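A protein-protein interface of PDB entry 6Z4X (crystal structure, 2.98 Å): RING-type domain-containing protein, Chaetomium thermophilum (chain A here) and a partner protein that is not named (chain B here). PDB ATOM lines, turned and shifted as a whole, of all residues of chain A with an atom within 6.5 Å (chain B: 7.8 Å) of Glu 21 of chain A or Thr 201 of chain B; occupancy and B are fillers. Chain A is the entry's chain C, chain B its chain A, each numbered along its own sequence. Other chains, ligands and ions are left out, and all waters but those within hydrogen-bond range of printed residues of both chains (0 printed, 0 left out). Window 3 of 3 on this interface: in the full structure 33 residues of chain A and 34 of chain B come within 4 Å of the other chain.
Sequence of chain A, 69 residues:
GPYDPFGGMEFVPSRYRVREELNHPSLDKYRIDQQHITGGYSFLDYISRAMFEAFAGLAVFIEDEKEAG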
ATOM      1  N   ARG A  17      12.178  16.176  14.097  1.00  0.00           N
ATOM      2  CA  ARG A  17      10.890  16.831  13.925  1.00  0.00           C
ATOM      3  C   ARG A  17      11.075  18.332  14.074  1.00  0.00           C
ATOM      4  O   ARG A  17      11.781  18.793  14.975  1.00  0.00           O
ATOM      5  CB  ARG A  17       9.853  16.324  14.939  1.00  0.00           C
ATOM      6  CG  ARG A  17      10.111  16.743  16.383  1.00  0.00           C
ATOM      7  CD  ARG A  17      11.372  16.101  16.935  1.00  0.00           C
ATOM      8  NE  ARG A  17      11.512  16.304  18.373  1.00  0.00           N
ATOM      9  CZ  ARG A  17      12.591  15.965  19.070  1.00  0.00           C
ATOM     10  NH1 ARG A  17      13.630  15.410  18.459  1.00  0.00           N
ATOM     11  NH2 ARG A  17      12.634  16.184  20.378  1.00  0.00           N
ATOM     12  N   ARG A  19       9.839  21.579  15.257  1.00  0.00           N
ATOM     13  CA  ARG A  19       8.905  22.112  16.237  1.00  0.00           C
ATOM     14  C   ARG A  19       9.020  23.630  16.315  1.00  0.00           C
ATOM     15  O   ARG A  19       9.930  24.246  15.754  1.00  0.00           O
ATOM     16  CB  ARG A  19       9.140  21.481  17.615  1.00  0.00           C
ATOM     17  CG  ARG A  19      10.601  21.287  17.977  1.00  0.00           C
ATOM     18  CD  ARG A  19      10.896  19.824  18.262  1.00  0.00           C
ATOM     19  NE  ARG A  19      11.333  19.610  19.639  1.00  0.00           N
ATOM     20  CZ  ARG A  19      12.604  19.595  20.022  1.00  0.00           C
ATOM     21  NH1 ARG A  19      12.914  19.394  21.297  1.00  0.00           N
ATOM     22  NH2 ARG A  19      13.568  19.781  19.129  1.00  0.00           N
ATOM     23  N   GLU A  20       8.067  24.230  17.033  1.00  0.00           N
ATOM     24  CA  GLU A  20       7.993  25.686  17.107  1.00  0.00           C
ATOM     25  C   GLU A  20       9.155  26.283  17.891  1.00  0.00           C
ATOM     26  O   GLU A  20       9.581  27.407  17.601  1.00  0.00           O
ATOM     27  CB  GLU A  20       6.665  26.107  17.738  1.00  0.00           C
ATOM     28  CG  GLU A  20       5.497  26.159  16.768  1.00  0.00           C
ATOM     29  CD  GLU A  20       4.221  26.661  17.421  1.00  0.00           C
ATOM     30  OE1 GLU A  20       4.309  27.289  18.498  1.00  0.00           O
ATOM     31  OE2 GLU A  20       3.131  26.436  16.852  1.00  0.00           O
ATOM     32  N   GLU A  21       9.682  25.556  18.879  1.00  0.00           N
ATOM     33  CA  GLU A  21      10.708  26.109  19.755  1.00  0.00           C
ATOM     34  C   GLU A  21      12.067  26.254  19.076  1.00  0.00           C
ATOM     35  O   GLU A  21      12.975  26.838  19.675  1.00  0.00           O
ATOM     36  CB  GLU A  21      10.848  25.241  21.007  1.00  0.00           C
ATOM     37  CG  GLU A  21      11.382  23.842  20.743  1.00  0.00           C
ATOM     38  CD  GLU A  21      11.416  22.984  21.995  1.00  0.00           C
ATOM     39  OE1 GLU A  21      10.777  21.911  21.998  1.00  0.00           O
ATOM     40  OE2 GLU A  21      12.072  23.388  22.980  1.00  0.00           O
ATOM     41  N   LEU A  22      12.229  25.745  17.858  1.00  0.00           N
ATOM     42  CA  LEU A  22      13.498  25.883  17.155  1.00  0.00           C
ATOM     43  C   LEU A  22      13.708  27.328  16.715  1.00  0.00           C
ATOM     44  O   LEU A  22      12.848  27.920  16.056  1.00  0.00           O
ATOM     45  CB  LEU A  22      13.535  24.947  15.948  1.00  0.00           C
ATOM     46  CG  LEU A  22      13.534  23.452  16.274  1.00  0.00           C
ATOM     47  CD1 LEU A  22      13.474  22.616  15.005  1.00  0.00           C
ATOM     48  CD2 LEU A  22      14.753  23.084  17.105  1.00  0.00           C
ATOM     49  N   ASN A  23      14.858  27.893  17.077  1.00  0.00           N
ATOM     50  CA  ASN A  23      15.216  29.244  16.663  1.00  0.00           C
ATOM     51  C   ASN A  23      16.701  29.450  16.927  1.00  0.00           C
ATOM     52  O   ASN A  23      17.320  28.709  17.697  1.00  0.00           O
ATOM     53  CB  ASN A  23      14.381  30.301  17.396  1.00  0.00           C
ATOM     54  CG  ASN A  23      14.426  31.656  16.713  1.00  0.00           C
ATOM     55  OD1 ASN A  23      14.660  31.751  15.507  1.00  0.00           O
ATOM     56  ND2 ASN A  23      14.200  32.713  17.483  1.00  0.00           N
ATOM     57  N   GLY B 194      21.523  24.100  11.980  1.00  0.00           N
ATOM     58  CA  GLY B 194      20.350  23.352  12.402  1.00  0.00           C
ATOM     59  C   GLY B 194      20.623  22.458  13.599  1.00  0.00           C
ATOM     60  O   GLY B 194      19.792  22.344  14.504  1.00  0.00           O
ATOM     61  N   ALA B 195      21.792  21.813  13.622  1.00  0.00           N
ATOM     62  CA  ALA B 195      22.153  20.997  14.777  1.00  0.00           C
ATOM     63  C   ALA B 195      22.327  21.857  16.022  1.00  0.00           C
ATOM     64  O   ALA B 195      21.934  21.452  17.123  1.00  0.00           O
ATOM     65  CB  ALA B 195      23.427  20.204  14.485  1.00  0.00           C
ATOM     66  N   ILE B 196      22.914  23.047  15.869  1.00  0.00           N
ATOM     67  CA  ILE B 196      23.042  23.953  17.007  1.00  0.00           C
ATOM     68  C   ILE B 196      21.666  24.364  17.514  1.00  0.00           C
ATOM     69  O   ILE B 196      21.436  24.450  18.726  1.00  0.00           O
ATOM     70  CB  ILE B 196      23.899  25.176  16.633  1.00  0.00           C
ATOM     71  CG1 ILE B 196      25.335  24.750  16.325  1.00  0.00           C
ATOM     72  CG2 ILE B 196      23.879  26.199  17.760  1.00  0.00           C
ATOM     73  CD1 ILE B 196      26.056  24.145  17.510  1.00  0.00           C
ATOM     74  N   MET B 197      20.728  24.619  16.599  1.00  0.00           N
ATOM     75  CA  MET B 197      19.367  24.937  17.022  1.00  0.00           C
ATOM     76  C   MET B 197      18.742  23.768  17.774  1.00  0.00           C
ATOM     77  O   MET B 197      18.079  23.961  18.800  1.00  0.00           O
ATOM     78  CB  MET B 197      18.507  25.314  15.817  1.00  0.00           C
ATOM     79  CG  MET B 197      18.914  26.598  15.125  1.00  0.00           C
ATOM     80  SD  MET B 197      17.910  26.868  13.655  1.00  0.00           S
ATOM     81  CE  MET B 197      16.327  26.255  14.224  1.00  0.00           C
ATOM     82  N   GLU B 198      18.938  22.546  17.275  1.00  0.00           N
ATOM     83  CA  GLU B 198      18.389  21.375  17.954  1.00  0.00           C
ATOM     84  C   GLU B 198      18.972  21.232  19.354  1.00  0.00           C
ATOM     85  O   GLU B 198      18.263  20.864  20.298  1.00  0.00           O
ATOM     86  CB  GLU B 198      18.648  20.115  17.131  1.00  0.00           C
ATOM     87  CG  GLU B 198      18.192  18.828  17.805  1.00  0.00           C
ATOM     88  CD  GLU B 198      16.718  18.845  18.163  1.00  0.00           C
ATOM     89  OE1 GLU B 198      15.916  19.390  17.375  1.00  0.00           O
ATOM     90  OE2 GLU B 198      16.361  18.312  19.235  1.00  0.00           O
ATOM     91  N   LEU B 199      20.266  21.520  19.508  1.00  0.00           N
ATOM     92  CA  LEU B 199      20.883  21.464  20.831  1.00  0.00           C
ATOM     93  C   LEU B 199      20.385  22.588  21.729  1.00  0.00           C
ATOM     94  O   LEU B 199      20.314  22.417  22.952  1.00  0.00           O
ATOM     95  CB  LEU B 199      22.406  21.523  20.709  1.00  0.00           C
ATOM     96  CG  LEU B 199      23.105  20.274  20.170  1.00  0.00           C
ATOM     97  CD1 LEU B 199      24.520  20.604  19.726  1.00  0.00           C
ATOM     98  CD2 LEU B 199      23.116  19.179  21.226  1.00  0.00           C
ATOM     99  N   SER B 200      20.040  23.738  21.147  1.00  0.00           N
ATOM    100  CA  SER B 200      19.569  24.866  21.942  1.00  0.00           C
ATOM    101  C   SER B 200      18.298  24.538  22.712  1.00  0.00           C
ATOM    102  O   SER B 200      18.019  25.182  23.730  1.00  0.00           O
ATOM    103  CB  SER B 200      19.330  26.080  21.041  1.00  0.00           C
ATOM    104  OG  SER B 200      20.532  26.504  20.421  1.00  0.00           O
ATOM    105  N   THR B 201      17.525  23.549  22.257  1.00  0.00           N
ATOM    106  CA  THR B 201      16.291  23.195  22.945  1.00  0.00           C
ATOM    107  C   THR B 201      16.552  22.452  24.247  1.00  0.00           C
ATOM    108  O   THR B 201      15.651  22.365  25.087  1.00  0.00           O
ATOM    109  CB  THR B 201      15.402  22.342  22.038  1.00  0.00           C
ATOM    110  OG1 THR B 201      15.985  21.043  21.882  1.00  0.00           O
ATOM    111  CG2 THR B 201      15.258  22.996  20.669  1.00  0.00           C
ATOM    112  N   LEU B 202      17.752  21.919  24.430  1.00  0.00           N
ATOM    113  CA  LEU B 202      18.066  21.205  25.659  1.00  0.00           C
ATOM    114  C   LEU B 202      18.284  22.201  26.793  1.00  0.00           C
ATOM    115  O   LEU B 202      19.025  23.177  26.621  1.00  0.00           O
ATOM    116  CB  LEU B 202      19.303  20.328  25.468  1.00  0.00           C
ATOM    117  CG  LEU B 202      19.113  18.995  24.738  1.00  0.00           C
ATOM    118  CD1 LEU B 202      18.439  19.184  23.386  1.00  0.00           C
ATOM    119  CD2 LEU B 202      20.447  18.286  24.570  1.00  0.00           C
ATOM    120  N   PRO B 203      17.650  22.004  27.954  1.00  0.00           N
ATOM    121  CA  PRO B 203      17.807  22.974  29.049  1.00  0.00           C
ATOM    122  C   PRO B 203      19.123  22.858  29.798  1.00  0.00           C
ATOM    123  O   PRO B 203      19.535  23.834  30.440  1.00  0.00           O
ATOM    124  CB  PRO B 203      16.619  22.660  29.976  1.00  0.00           C
ATOM    125  CG  PRO B 203      15.726  21.720  29.193  1.00  0.00           C
ATOM    126  CD  PRO B 203      16.627  20.993  28.255  1.00  0.00           C
ATOM    127  N   ASP B 204      19.793  21.706  29.744  1.00  0.00           N
ATOM    128  CA  ASP B 204      21.033  21.531  30.492  1.00  0.00           C
ATOM    129  C   ASP B 204      22.219  22.217  29.824  1.00  0.00           C
ATOM    130  O   ASP B 204      23.150  22.643  30.515  1.00  0.00           O
ATOM    131  CB  ASP B 204      21.325  20.042  30.682  1.00  0.00           C
ATOM    132  CG  ASP B 204      21.073  19.234  29.423  1.00  0.00           C
ATOM    133  OD1 ASP B 204      20.549  19.806  28.444  1.00  0.00           O
ATOM    134  OD2 ASP B 204      21.399  18.028  29.414  1.00  0.00           O
ATOM    135  N   VAL B 205      22.207  22.332  28.495  1.00  0.00           N
ATOM    136  CA  VAL B 205      23.333  22.932  27.788  1.00  0.00           C
ATOM    137  C   VAL B 205      23.364  24.437  28.033  1.00  0.00           C
ATOM    138  O   VAL B 205      22.325  25.091  28.196  1.00  0.00           O
ATOM    139  CB  VAL B 205      23.257  22.616  26.284  1.00  0.00           C
ATOM    140  CG1 VAL B 205      23.133  21.116  26.067  1.00  0.00           C
ATOM    141  CG2 VAL B 205      22.090  23.354  25.647  1.00  0.00           C
ATOM    142  N   LEU B 210      27.629  26.537  23.671  1.00  0.00           N
ATOM    143  CA  LEU B 210      27.095  26.281  22.338  1.00  0.00           C
ATOM    144  C   LEU B 210      27.636  27.280  21.324  1.00  0.00           C
ATOM    145  O   LEU B 210      27.951  26.910  20.190  1.00  0.00           O
ATOM    146  CB  LEU B 210      25.567  26.324  22.366  1.00  0.00           C
ATOM    147  CG  LEU B 210      24.859  25.011  22.692  1.00  0.00           C
ATOM    148  CD1 LEU B 210      23.353  25.209  22.671  1.00  0.00           C
ATOM    149  CD2 LEU B 210      25.277  23.934  21.712  1.00  0.00           C
ATOM    150  N   LEU B 255      23.865  15.004  21.051  1.00  0.00           N
ATOM    151  CA  LEU B 255      22.876  15.047  19.979  1.00  0.00           C
ATOM    152  C   LEU B 255      22.612  13.653  19.421  1.00  0.00           C
ATOM    153  O   LEU B 255      21.453  13.270  19.205  1.00  0.00           O
ATOM    154  CB  LEU B 255      23.343  15.997  18.875  1.00  0.00           C
ATOM    155  CG  LEU B 255      22.327  16.332  17.782  1.00  0.00           C
ATOM    156  CD1 LEU B 255      20.994  16.726  18.390  1.00  0.00           C
ATOM    157  CD2 LEU B 255      22.857  17.440  16.883  1.00  0.00           C
ATOM    158  N   ASP B 258      20.606  11.676  21.927  1.00  0.00           N
ATOM    159  CA  ASP B 258      19.210  12.099  21.931  1.00  0.00           C
ATOM    160  C   ASP B 258      18.464  11.532  20.732  1.00  0.00           C
ATOM    161  O   ASP B 258      17.327  11.064  20.864  1.00  0.00           O
ATOM    162  CB  ASP B 258      19.119  13.625  21.944  1.00  0.00           C
ATOM    163  CG  ASP B 258      19.359  14.214  23.321  1.00  0.00           C
ATOM    164  OD1 ASP B 258      19.681  13.446  24.252  1.00  0.00           O
ATOM    165  OD2 ASP B 258      19.224  15.447  23.469  1.00  0.00           O
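NH2 of Arg 19 of chain A is in salt-bridge range of OE1 of Glu 198 of chain B.
The side-chain hydroxyl (OG1) of Thr 201 of chain B lies within hydrogen-bond range of the backbone carbonyl oxygen (O) of Glu 198 of chain B, 2.8 Å away.
The guanidinium group of Arg 19 of chain A lies within salt-bridge range of the side-chain carboxylate of Glu 21 of chain A (3.3 Å).
Among the printed residues, pairs that only touch across the chains: Arg 19 of chain A with Thr 201 of chain B, Glu 21 of chain A with Thr 201 of chain B, Leu 22 of chain A with Met 197 of chain B, Leu 22 of chain A with Glu 198 of chain B, Leu 22 of chain A with Thr 201 of chain B and Asn 23 of chain A with Met 197 of chain B.
Of chain B, only Thr 201 comes within 4 Å of Glu 21 of chain A.
Thr 201 of chain B touches three residues of chain A.
Of the printed residues of chain B, Arg 19 of chain A touches Glu 198 and Thr 201.
Printed residues of chain A within 4 Å of Met 197 of chain B: Leu 22 (3.5 Å) and Asn 23 (3.6 Å).
Of the printed residues of chain B, Asn 23 of chain A touches Met 197.
Of the printed residues of chain A, Glu 198 of chain B touches Arg 19 (3.0 Å) and Leu 22 (3.9 Å).
Asp 204 of chain B touches none of the printed residues of chain A.
The nearest residue of chain B that does not touch Glu 21 of chain A is Met 197 of chain B (5.9 Å).
The nearest printed residue of chain A that does not touch Thr 201 of chain B is Asn 23 of chain A (6.1 Å).
The nearest printed residue of chain A that does not touch Glu 198 of chain B is Arg 17 of chain A (4.1 Å).
Of the 6 printed residues of chain A, 4 touch a printed residue of chain B.
Printed residues of chain A that touch a printed residue of chain B: Arg 19, Glu 21, Leu 22 and Asn 23.
Hydrophobic or aromatic side chains of chain A within 4 Å of the printed part of chain B: Leu 22.
Of the 15 printed residues of chain B, 3 touch a printed residue of chain A.
Among the printed residues, 7 pairs touch across the chains.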
